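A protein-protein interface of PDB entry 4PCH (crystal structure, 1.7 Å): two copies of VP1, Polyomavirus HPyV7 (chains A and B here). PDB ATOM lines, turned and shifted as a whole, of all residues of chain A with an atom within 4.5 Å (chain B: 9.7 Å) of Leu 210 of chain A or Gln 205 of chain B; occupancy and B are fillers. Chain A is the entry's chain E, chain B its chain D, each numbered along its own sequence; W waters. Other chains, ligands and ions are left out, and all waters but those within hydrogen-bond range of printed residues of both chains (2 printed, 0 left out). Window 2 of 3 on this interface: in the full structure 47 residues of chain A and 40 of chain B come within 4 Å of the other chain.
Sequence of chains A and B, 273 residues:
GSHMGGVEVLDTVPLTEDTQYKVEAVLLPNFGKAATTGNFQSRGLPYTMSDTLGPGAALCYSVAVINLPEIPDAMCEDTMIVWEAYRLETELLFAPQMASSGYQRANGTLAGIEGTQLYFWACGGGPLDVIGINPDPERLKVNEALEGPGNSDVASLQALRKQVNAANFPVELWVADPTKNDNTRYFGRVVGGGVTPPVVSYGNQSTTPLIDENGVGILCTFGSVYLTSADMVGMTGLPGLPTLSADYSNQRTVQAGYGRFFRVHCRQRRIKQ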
ATOM      1  N   ALA A  85     -27.470  28.947  20.577  1.00  0.00           N
ATOM      2  CA  ALA A  85     -27.922  28.202  21.750  1.00  0.00           C
ATOM      3  C   ALA A  85     -27.048  28.599  22.941  1.00  0.00           C
ATOM      4  O   ALA A  85     -25.837  28.345  22.914  1.00  0.00           O
ATOM      5  CB  ALA A  85     -27.851  26.699  21.512  1.00  0.00           C
ATOM      6  N   TYR A  86     -27.649  29.219  23.967  1.00  0.00           N
ATOM      7  CA  TYR A  86     -26.879  29.857  25.049  1.00  0.00           C
ATOM      8  C   TYR A  86     -27.036  29.149  26.407  1.00  0.00           C
ATOM      9  O   TYR A  86     -26.263  29.403  27.331  1.00  0.00           O
ATOM     10  CB  TYR A  86     -27.234  31.347  25.177  1.00  0.00           C
ATOM     11  CG  TYR A  86     -28.690  31.610  25.484  1.00  0.00           C
ATOM     12  CD1 TYR A  86     -29.621  31.680  24.469  1.00  0.00           C
ATOM     13  CD2 TYR A  86     -29.132  31.788  26.792  1.00  0.00           C
ATOM     14  CE1 TYR A  86     -30.955  31.906  24.737  1.00  0.00           C
ATOM     15  CE2 TYR A  86     -30.469  32.015  27.072  1.00  0.00           C
ATOM     16  CZ  TYR A  86     -31.375  32.074  26.031  1.00  0.00           C
ATOM     17  OH  TYR A  86     -32.709  32.312  26.256  1.00  0.00           O
ATOM     18  N   ARG A  87     -28.000  28.238  26.490  1.00  0.00           N
ATOM     19  CA  ARG A  87     -28.317  27.549  27.737  1.00  0.00           C
ATOM     20  C   ARG A  87     -29.061  26.269  27.421  1.00  0.00           C
ATOM     21  O   ARG A  87     -29.811  26.205  26.442  1.00  0.00           O
ATOM     22  CB  ARG A  87     -29.192  28.479  28.586  1.00  0.00           C
ATOM     23  CG  ARG A  87     -29.971  27.813  29.711  1.00  0.00           C
ATOM     24  CD  ARG A  87     -30.530  28.849  30.683  1.00  0.00           C
ATOM     25  NE  ARG A  87     -29.568  29.920  30.950  1.00  0.00           N
ATOM     26  CZ  ARG A  87     -28.502  29.830  31.749  1.00  0.00           C
ATOM     27  NH1 ARG A  87     -28.222  28.700  32.398  1.00  0.00           N
ATOM     28  NH2 ARG A  87     -27.696  30.880  31.899  1.00  0.00           N
ATOM     29  N   LEU A  88     -28.846  25.232  28.217  1.00  0.00           N
ATOM     30  CA  LEU A  88     -29.683  24.040  28.099  1.00  0.00           C
ATOM     31  C   LEU A  88     -29.978  23.426  29.450  1.00  0.00           C
ATOM     32  O   LEU A  88     -29.246  23.656  30.429  1.00  0.00           O
ATOM     33  CB  LEU A  88     -29.078  22.993  27.133  1.00  0.00           C
ATOM     34  CG  LEU A  88     -27.823  22.212  27.543  1.00  0.00           C
ATOM     35  CD1 LEU A  88     -28.028  21.138  28.641  1.00  0.00           C
ATOM     36  CD2 LEU A  88     -27.191  21.552  26.324  1.00  0.00           C
ATOM     37  N   TRP A 121     -22.987  14.026  27.492  1.00  0.00           N
ATOM     38  CA  TRP A 121     -23.846  14.844  26.627  1.00  0.00           C
ATOM     39  C   TRP A 121     -23.036  15.857  25.811  1.00  0.00           C
ATOM     40  O   TRP A 121     -21.930  16.252  26.203  1.00  0.00           O
ATOM     41  CB  TRP A 121     -24.916  15.574  27.445  1.00  0.00           C
ATOM     42  CG  TRP A 121     -24.385  16.596  28.419  1.00  0.00           C
ATOM     43  CD1 TRP A 121     -24.198  16.431  29.757  1.00  0.00           C
ATOM     44  CD2 TRP A 121     -23.994  17.938  28.121  1.00  0.00           C
ATOM     45  NE1 TRP A 121     -23.710  17.573  30.312  1.00  0.00           N
ATOM     46  CE2 TRP A 121     -23.562  18.515  29.331  1.00  0.00           C
ATOM     47  CE3 TRP A 121     -23.936  18.703  26.941  1.00  0.00           C
ATOM     48  CZ2 TRP A 121     -23.101  19.823  29.410  1.00  0.00           C
ATOM     49  CZ3 TRP A 121     -23.486  19.996  27.015  1.00  0.00           C
ATOM     50  CH2 TRP A 121     -23.070  20.554  28.247  1.00  0.00           C
ATOM     51  N   CYS A 123     -23.842  19.318  22.853  1.00  0.00           N
ATOM     52  CA  CYS A 123     -24.752  20.157  22.091  1.00  0.00           C
ATOM     53  C   CYS A 123     -23.876  21.064  21.234  1.00  0.00           C
ATOM     54  O   CYS A 123     -22.980  21.741  21.740  1.00  0.00           O
ATOM     55  CB  CYS A 123     -25.614  20.990  23.038  1.00  0.00           C
ATOM     56  SG  CYS A 123     -26.661  22.253  22.295  1.00  0.00           S
ATOM     57  N   ARG A 185     -20.401  22.206  22.897  1.00  0.00           N
ATOM     58  CA  ARG A 185     -20.025  21.962  24.312  1.00  0.00           C
ATOM     59  C   ARG A 185     -20.306  20.516  24.651  1.00  0.00           C
ATOM     60  O   ARG A 185     -21.330  19.953  24.247  1.00  0.00           O
ATOM     61  CB  ARG A 185     -20.792  22.876  25.256  1.00  0.00           C
ATOM     62  CG  ARG A 185     -20.806  24.343  24.858  1.00  0.00           C
ATOM     63  CD  ARG A 185     -19.449  24.989  24.642  1.00  0.00           C
ATOM     64  NE  ARG A 185     -19.662  26.416  24.416  1.00  0.00           N
ATOM     65  CZ  ARG A 185     -19.273  27.108  23.348  1.00  0.00           C
ATOM     66  NH1 ARG A 185     -18.588  26.544  22.344  1.00  0.00           N
ATOM     67  NH2 ARG A 185     -19.582  28.400  23.260  1.00  0.00           N
ATOM     68  N   THR A 208     -27.651  24.425  32.544  1.00  0.00           N
ATOM     69  CA  THR A 208     -26.283  24.409  32.064  1.00  0.00           C
ATOM     70  C   THR A 208     -26.075  25.535  31.041  1.00  0.00           C
ATOM     71  O   THR A 208     -26.679  25.502  29.964  1.00  0.00           O
ATOM     72  CB  THR A 208     -26.009  23.059  31.394  1.00  0.00           C
ATOM     73  OG1 THR A 208     -26.217  22.007  32.356  1.00  0.00           O
ATOM     74  CG2 THR A 208     -24.596  23.005  30.824  1.00  0.00           C
ATOM     75  N   PRO A 209     -25.225  26.533  31.366  1.00  0.00           N
ATOM     76  CA  PRO A 209     -24.921  27.563  30.353  1.00  0.00           C
ATOM     77  C   PRO A 209     -23.978  27.049  29.255  1.00  0.00           C
ATOM     78  O   PRO A 209     -23.127  26.192  29.510  1.00  0.00           O
ATOM     79  CB  PRO A 209     -24.271  28.688  31.156  1.00  0.00           C
ATOM     80  CG  PRO A 209     -23.793  28.066  32.438  1.00  0.00           C
ATOM     81  CD  PRO A 209     -24.469  26.733  32.620  1.00  0.00           C
ATOM     82  N   LEU A 210     -24.124  27.601  28.050  1.00  0.00           N
ATOM     83  CA  LEU A 210     -23.330  27.177  26.909  1.00  0.00           C
ATOM     84  C   LEU A 210     -22.436  28.296  26.376  1.00  0.00           C
ATOM     85  O   LEU A 210     -21.782  28.128  25.348  1.00  0.00           O
ATOM     86  CB  LEU A 210     -24.259  26.663  25.798  1.00  0.00           C
ATOM     87  CG  LEU A 210     -25.120  25.449  26.136  1.00  0.00           C
ATOM     88  CD1 LEU A 210     -26.204  25.193  25.100  1.00  0.00           C
ATOM     89  CD2 LEU A 210     -24.255  24.210  26.307  1.00  0.00           C
ATOM     90  N   ILE A 211     -22.399  29.437  27.067  1.00  0.00           N
ATOM     91  CA  ILE A 211     -21.609  30.576  26.604  1.00  0.00           C
ATOM     92  C   ILE A 211     -20.138  30.489  26.985  1.00  0.00           C
ATOM     93  O   ILE A 211     -19.786  30.039  28.081  1.00  0.00           O
ATOM     94  CB  ILE A 211     -22.160  31.933  27.106  1.00  0.00           C
ATOM     95  CG1 ILE A 211     -22.179  31.996  28.644  1.00  0.00           C
ATOM     96  CG2 ILE A 211     -23.527  32.207  26.488  1.00  0.00           C
ATOM     97  CD1 ILE A 211     -22.535  33.340  29.223  1.00  0.00           C
ATOM     98  N   ASP A 212     -19.285  30.941  26.074  1.00  0.00           N
ATOM     99  CA  ASP A 212     -17.834  30.921  26.270  1.00  0.00           C
ATOM    100  C   ASP A 212     -17.364  32.179  27.021  1.00  0.00           C
ATOM    101  O   ASP A 212     -18.193  32.924  27.538  1.00  0.00           O
ATOM    102  CB  ASP A 212     -17.133  30.753  24.910  1.00  0.00           C
ATOM    103  CG  ASP A 212     -17.311  31.976  23.978  1.00  0.00           C
ATOM    104  OD1 ASP A 212     -17.742  33.062  24.423  1.00  0.00           O
ATOM    105  OD2 ASP A 212     -17.019  31.834  22.779  1.00  0.00           O
ATOM    106  N   VAL A 216     -20.504  34.109  24.093  1.00  0.00           N
ATOM    107  CA  VAL A 216     -21.055  33.530  22.863  1.00  0.00           C
ATOM    108  C   VAL A 216     -21.341  32.028  23.035  1.00  0.00           C
ATOM    109  O   VAL A 216     -20.475  31.240  23.462  1.00  0.00           O
ATOM    110  CB  VAL A 216     -20.098  33.745  21.656  1.00  0.00           C
ATOM    111  CG1 VAL A 216     -20.717  33.204  20.361  1.00  0.00           C
ATOM    112  CG2 VAL A 216     -19.743  35.222  21.496  1.00  0.00           C
ATOM    113  N   GLY A 217     -22.574  31.647  22.713  1.00  0.00           N
ATOM    114  CA  GLY A 217     -23.010  30.270  22.767  1.00  0.00           C
ATOM    115  C   GLY A 217     -22.722  29.540  21.465  1.00  0.00           C
ATOM    116  O   GLY A 217     -21.887  29.971  20.678  1.00  0.00           O
ATOM    117  N   ILE A 218     -23.432  28.428  21.263  1.00  0.00           N
ATOM    118  CA  ILE A 218     -23.321  27.600  20.062  1.00  0.00           C
ATOM    119  C   ILE A 218     -23.980  28.306  18.898  1.00  0.00           C
ATOM    120  O   ILE A 218     -25.158  28.625  18.953  1.00  0.00           O
ATOM    121  CB  ILE A 218     -24.019  26.226  20.300  1.00  0.00           C
ATOM    122  CG1 ILE A 218     -23.385  25.480  21.484  1.00  0.00           C
ATOM    123  CG2 ILE A 218     -24.041  25.379  19.046  1.00  0.00           C
ATOM    124  CD1 ILE A 218     -21.882  25.327  21.435  1.00  0.00           C
ATOM    125  N   ARG B  87      -3.713  31.305  31.892  1.00  0.00           N
ATOM    126  CA  ARG B  87      -4.888  30.449  31.916  1.00  0.00           C
ATOM    127  C   ARG B  87      -4.635  29.199  31.074  1.00  0.00           C
ATOM    128  O   ARG B  87      -3.920  29.249  30.077  1.00  0.00           O
ATOM    129  CB  ARG B  87      -6.084  31.217  31.368  1.00  0.00           C
ATOM    130  CG  ARG B  87      -7.395  30.473  31.360  1.00  0.00           C
ATOM    131  CD  ARG B  87      -8.557  31.443  31.181  1.00  0.00           C
ATOM    132  NE  ARG B  87      -8.722  32.288  32.366  1.00  0.00           N
ATOM    133  CZ  ARG B  87      -9.230  31.879  33.535  1.00  0.00           C
ATOM    134  NH1 ARG B  87      -9.649  30.632  33.702  1.00  0.00           N
ATOM    135  NH2 ARG B  87      -9.322  32.730  34.551  1.00  0.00           N
ATOM    136  N   LEU B  88      -5.172  28.064  31.507  1.00  0.00           N
ATOM    137  CA  LEU B  88      -5.170  26.869  30.656  1.00  0.00           C
ATOM    138  C   LEU B  88      -6.447  26.073  30.788  1.00  0.00           C
ATOM    139  O   LEU B  88      -7.169  26.194  31.786  1.00  0.00           O
ATOM    140  CB  LEU B  88      -3.931  25.992  30.894  1.00  0.00           C
ATOM    141  CG  LEU B  88      -3.771  25.167  32.179  1.00  0.00           C
ATOM    142  CD1 LEU B  88      -4.661  23.936  32.223  1.00  0.00           C
ATOM    143  CD2 LEU B  88      -2.328  24.723  32.345  1.00  0.00           C
ATOM    144  N   GLU B  89      -6.714  25.262  29.764  1.00  0.00           N
ATOM    145  CA  GLU B  89      -7.681  24.180  29.841  1.00  0.00           C
ATOM    146  C   GLU B  89      -6.913  22.869  29.703  1.00  0.00           C
ATOM    147  O   GLU B  89      -5.975  22.777  28.913  1.00  0.00           O
ATOM    148  CB  GLU B  89      -8.741  24.286  28.749  1.00  0.00           C
ATOM    149  CG  GLU B  89      -9.664  25.489  28.915  1.00  0.00           C
ATOM    150  CD  GLU B  89      -9.056  26.776  28.406  1.00  0.00           C
ATOM    151  OE1 GLU B  89      -8.693  26.821  27.215  1.00  0.00           O
ATOM    152  OE2 GLU B  89      -8.964  27.758  29.177  1.00  0.00           O
ATOM    153  N   THR B  90      -7.291  21.869  30.481  1.00  0.00           N
ATOM    154  CA  THR B  90      -6.712  20.528  30.332  1.00  0.00           C
ATOM    155  C   THR B  90      -7.803  19.481  30.503  1.00  0.00           C
ATOM    156  O   THR B  90      -8.673  19.629  31.360  1.00  0.00           O
ATOM    157  CB  THR B  90      -5.529  20.271  31.293  1.00  0.00           C
ATOM    158  OG1 THR B  90      -4.959  18.980  31.029  1.00  0.00           O
ATOM    159  CG2 THR B  90      -5.958  20.332  32.787  1.00  0.00           C
ATOM    160  N   GLU B  91      -7.776  18.443  29.676  1.00  0.00           N
ATOM    161  CA  GLU B  91      -8.717  17.332  29.832  1.00  0.00           C
ATOM    162  C   GLU B  91      -8.080  15.993  29.493  1.00  0.00           C
ATOM    163  O   GLU B  91      -7.223  15.905  28.617  1.00  0.00           O
ATOM    164  CB  GLU B  91     -10.008  17.548  29.020  1.00  0.00           C
ATOM    165  CG  GLU B  91      -9.880  17.887  27.555  1.00  0.00           C
ATOM    166  CD  GLU B  91     -11.224  18.231  26.889  1.00  0.00           C
ATOM    167  OE1 GLU B  91     -11.430  19.438  26.572  1.00  0.00           O
ATOM    168  OE2 GLU B  91     -12.058  17.304  26.647  1.00  0.00           O
ATOM    169  N   TYR B 202     -14.396  14.705  32.095  1.00  0.00           N
ATOM    170  CA  TYR B 202     -13.818  15.548  31.045  1.00  0.00           C
ATOM    171  C   TYR B 202     -14.896  16.371  30.377  1.00  0.00           C
ATOM    172  O   TYR B 202     -16.083  16.080  30.469  1.00  0.00           O
ATOM    173  CB  TYR B 202     -13.090  14.707  29.986  1.00  0.00           C
ATOM    174  CG  TYR B 202     -13.988  13.711  29.287  1.00  0.00           C
ATOM    175  CD1 TYR B 202     -14.730  14.063  28.174  1.00  0.00           C
ATOM    176  CD2 TYR B 202     -14.108  12.393  29.757  1.00  0.00           C
ATOM    177  CE1 TYR B 202     -15.565  13.153  27.550  1.00  0.00           C
ATOM    178  CE2 TYR B 202     -14.937  11.486  29.131  1.00  0.00           C
ATOM    179  CZ  TYR B 202     -15.661  11.857  28.035  1.00  0.00           C
ATOM    180  OH  TYR B 202     -16.502  10.975  27.412  1.00  0.00           O
ATOM    181  N   GLY B 203     -14.472  17.414  29.679  1.00  0.00           N
ATOM    182  CA  GLY B 203     -15.404  18.307  29.005  1.00  0.00           C
ATOM    183  C   GLY B 203     -14.630  19.480  28.434  1.00  0.00           C
ATOM    184  O   GLY B 203     -13.431  19.600  28.656  1.00  0.00           O
ATOM    185  N   ASN B 204     -15.288  20.361  27.711  1.00  0.00           N
ATOM    186  CA  ASN B 204     -14.548  21.453  27.082  1.00  0.00           C
ATOM    187  C   ASN B 204     -15.013  22.813  27.570  1.00  0.00           C
ATOM    188  O   ASN B 204     -14.876  23.808  26.862  1.00  0.00           O
ATOM    189  CB  ASN B 204     -14.597  21.324  25.551  1.00  0.00           C
ATOM    190  CG  ASN B 204     -15.982  21.548  24.986  1.00  0.00           C
ATOM    191  OD1 ASN B 204     -16.983  21.520  25.703  1.00  0.00           O
ATOM    192  ND2 ASN B 204     -16.044  21.798  23.681  1.00  0.00           N
ATOM    193  N   GLN B 205     -15.550  22.854  28.797  1.00  0.00           N
ATOM    194  CA  GLN B 205     -15.985  24.120  29.383  1.00  0.00           C
ATOM    195  C   GLN B 205     -15.210  24.536  30.636  1.00  0.00           C
ATOM    196  O   GLN B 205     -15.321  25.672  31.063  1.00  0.00           O
ATOM    197  CB  GLN B 205     -17.471  24.069  29.697  1.00  0.00           C
ATOM    198  CG  GLN B 205     -18.367  23.969  28.490  1.00  0.00           C
ATOM    199  CD  GLN B 205     -19.820  23.892  28.884  1.00  0.00           C
ATOM    200  OE1 GLN B 205     -20.267  22.883  29.427  1.00  0.00           O
ATOM    201  NE2 GLN B 205     -20.567  24.959  28.621  1.00  0.00           N
ATOM    202  N   SER B 206     -14.422  23.655  31.224  1.00  0.00           N
ATOM    203  CA  SER B 206     -13.726  24.015  32.458  1.00  0.00           C
ATOM    204  C   SER B 206     -12.427  24.711  32.102  1.00  0.00           C
ATOM    205  O   SER B 206     -11.885  24.525  31.014  1.00  0.00           O
ATOM    206  CB  SER B 206     -13.483  22.793  33.344  1.00  0.00           C
ATOM    207  OG  SER B 206     -12.403  22.022  32.864  1.00  0.00           O
ATOM    208  N   THR B 207     -11.952  25.559  32.996  1.00  0.00           N
ATOM    209  CA  THR B 207     -10.720  26.282  32.755  1.00  0.00           C
ATOM    210  C   THR B 207     -10.011  26.479  34.069  1.00  0.00           C
ATOM    211  O   THR B 207     -10.653  26.451  35.121  1.00  0.00           O
ATOM    212  CB  THR B 207     -10.989  27.623  32.060  1.00  0.00           C
ATOM    213  OG1 THR B 207      -9.741  28.240  31.719  1.00  0.00           O
ATOM    214  CG2 THR B 207     -11.842  28.556  32.952  1.00  0.00           C
ATOM    215  N   THR B 208      -8.695  26.655  33.991  1.00  0.00           N
ATOM    216  CA  THR B 208      -7.829  26.752  35.159  1.00  0.00           C
ATOM    217  C   THR B 208      -6.962  28.008  35.091  1.00  0.00           C
ATOM    218  O   THR B 208      -6.063  28.077  34.253  1.00  0.00           O
ATOM    219  CB  THR B 208      -6.885  25.531  35.220  1.00  0.00           C
ATOM    220  OG1 THR B 208      -7.648  24.315  35.236  1.00  0.00           O
ATOM    221  CG2 THR B 208      -6.006  25.598  36.455  1.00  0.00           C
ATOM    222  N   PHE B 261      -5.023  16.542  26.903  1.00  0.00           N
ATOM    223  CA  PHE B 261      -5.105  17.768  26.131  1.00  0.00           C
ATOM    224  C   PHE B 261      -4.762  18.957  27.003  1.00  0.00           C
ATOM    225  O   PHE B 261      -5.179  18.995  28.169  1.00  0.00           O
ATOM    226  CB  PHE B 261      -6.544  17.921  25.605  1.00  0.00           C
ATOM    227  CG  PHE B 261      -6.824  19.236  24.946  1.00  0.00           C
ATOM    228  CD1 PHE B 261      -6.432  19.460  23.624  1.00  0.00           C
ATOM    229  CD2 PHE B 261      -7.519  20.246  25.620  1.00  0.00           C
ATOM    230  CE1 PHE B 261      -6.682  20.666  23.014  1.00  0.00           C
ATOM    231  CE2 PHE B 261      -7.770  21.458  24.998  1.00  0.00           C
ATOM    232  CZ  PHE B 261      -7.363  21.660  23.697  1.00  0.00           C
ATOM    233  N   ARG B 263      -4.737  23.428  26.477  1.00  0.00           N
ATOM    234  CA  ARG B 263      -4.787  24.689  25.747  1.00  0.00           C
ATOM    235  C   ARG B 263      -4.243  25.719  26.707  1.00  0.00           C
ATOM    236  O   ARG B 263      -4.792  25.891  27.802  1.00  0.00           O
ATOM    237  CB  ARG B 263      -6.206  25.074  25.299  1.00  0.00           C
ATOM    238  CG  ARG B 263      -6.232  26.314  24.410  1.00  0.00           C
ATOM    239  CD  ARG B 263      -7.631  26.777  24.022  1.00  0.00           C
ATOM    240  NE  ARG B 263      -8.409  25.752  23.319  1.00  0.00           N
ATOM    241  CZ  ARG B 263      -9.266  24.905  23.901  1.00  0.00           C
ATOM    242  NH1 ARG B 263      -9.919  24.006  23.176  1.00  0.00           N
ATOM    243  NH2 ARG B 263      -9.482  24.938  25.212  1.00  0.00           N
ATOM    244  N   HIS B 265      -3.146  29.674  27.417  1.00  0.00           N
ATOM    245  CA  HIS B 265      -3.383  31.039  26.950  1.00  0.00           C
ATOM    246  C   HIS B 265      -2.291  31.989  27.429  1.00  0.00           C
ATOM    247  O   HIS B 265      -1.989  32.042  28.620  1.00  0.00           O
ATOM    248  CB  HIS B 265      -4.740  31.549  27.436  1.00  0.00           C
ATOM    249  CG  HIS B 265      -5.887  30.683  27.026  1.00  0.00           C
ATOM    250  ND1 HIS B 265      -6.711  30.990  25.960  1.00  0.00           N
ATOM    251  CD2 HIS B 265      -6.339  29.508  27.528  1.00  0.00           C
ATOM    252  CE1 HIS B 265      -7.624  30.040  25.833  1.00  0.00           C
ATOM    253  NE2 HIS B 265      -7.420  29.133  26.771  1.00  0.00           N
HETATM  254  O   HOH W   1     -19.528  27.097  27.450  1.00  0.00           O
HETATM  255  O   HOH W   2     -16.472  24.653  22.226  1.00  0.00           O
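The side-chain amide nitrogen of Gln 205 of chain B is in hydrogen-bond range of the backbone carbonyl oxygen of Pro 209 of chain A (3.0 Å).
O of Leu 210 of chain A sits at hydrogen-bond distance from NE of Arg 185 of chain A, 2.9 Å away.
O of Cys 123 of chain A lies within hydrogen-bond range of N of Arg 185 of chain A (2.9 Å).
NH2 of Arg 185 of chain A is in hydrogen-bond range of O of Val 216 of chain A (3.0 Å).
N of Leu 210 of chain A sits at hydrogen-bond distance from O of Tyr 86 of chain A.
Trp 121 of chain A touches Gln 205 of chain B (CH2 to OE1, 3.8 Å).
Arg 185 of chain A touches Asn 204 of chain B.
Arg 185 of chain A touches Gln 205 of chain B.
CA of Leu 210 of chain A touches NE2 of Gln 205 of chain B, 3.9 Å away.
Printed residues of chain B within 4 Å of Trp 121 of chain A: Gln 205 (3.8 Å).
Of chain B, only Asn 204 (3.4 Å) and Gln 205 (3.8 Å) come within 4 Å of Arg 185 of chain A.
Pro 209 of chain A touches one residue of chain B.
Leu 210 of chain A touches just one residue of chain B: Gln 205 (3.9 Å).
No residue of chain B comes within 4 Å of Gly 217 of chain A.
Leu 88 of chain B touches none of the printed residues of chain A.
Of the printed residues of chain A, Asn 204 of chain B touches Arg 185.
Printed residues of chain A within 4 Å of Gln 205 of chain B: Trp 121, Arg 185, Pro 209 and Leu 210.
The nearest residue of chain B that does not touch Leu 210 of chain A is Asn 204 of chain B (7.8 Å).
The nearest printed residue of chain B that does not touch Trp 121 of chain A is Asn 204 of chain B (6.7 Å).
Printed residues of chain B that touch a printed residue of chain A: Asn 204 and Gln 205.
Of the 15 printed residues of chain A, 4 touch a printed residue of chain B.
Hydrophobic or aromatic side chains of chain A that line the printed part of chain B: Trp 121.
Among the printed residues, 5 pairs touch across the chains.
Among the printed residues, no Asp or Glu carboxylate lies within 4 Å of a Lys or Arg side-chain nitrogen of the other chain.
Positions printed for both chains: 87, 88 and 208.
Water W1 lies within hydrogen-bond range of the side-chain amide nitrogen of Gln 205 of chain B (2.6 Å), the backbone carbonyl oxygen of Ile 211 of chain A (3.0 Å), the guanidinium group of Arg 185 of chain A (3.1 Å) and the backbone carbonyl oxygen of Leu 210 of chain A (3.2 Å).
Water W2 lies within hydrogen-bond range of NH1 of Arg 185 of chain A and ND2 of Asn 204 of chain B.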
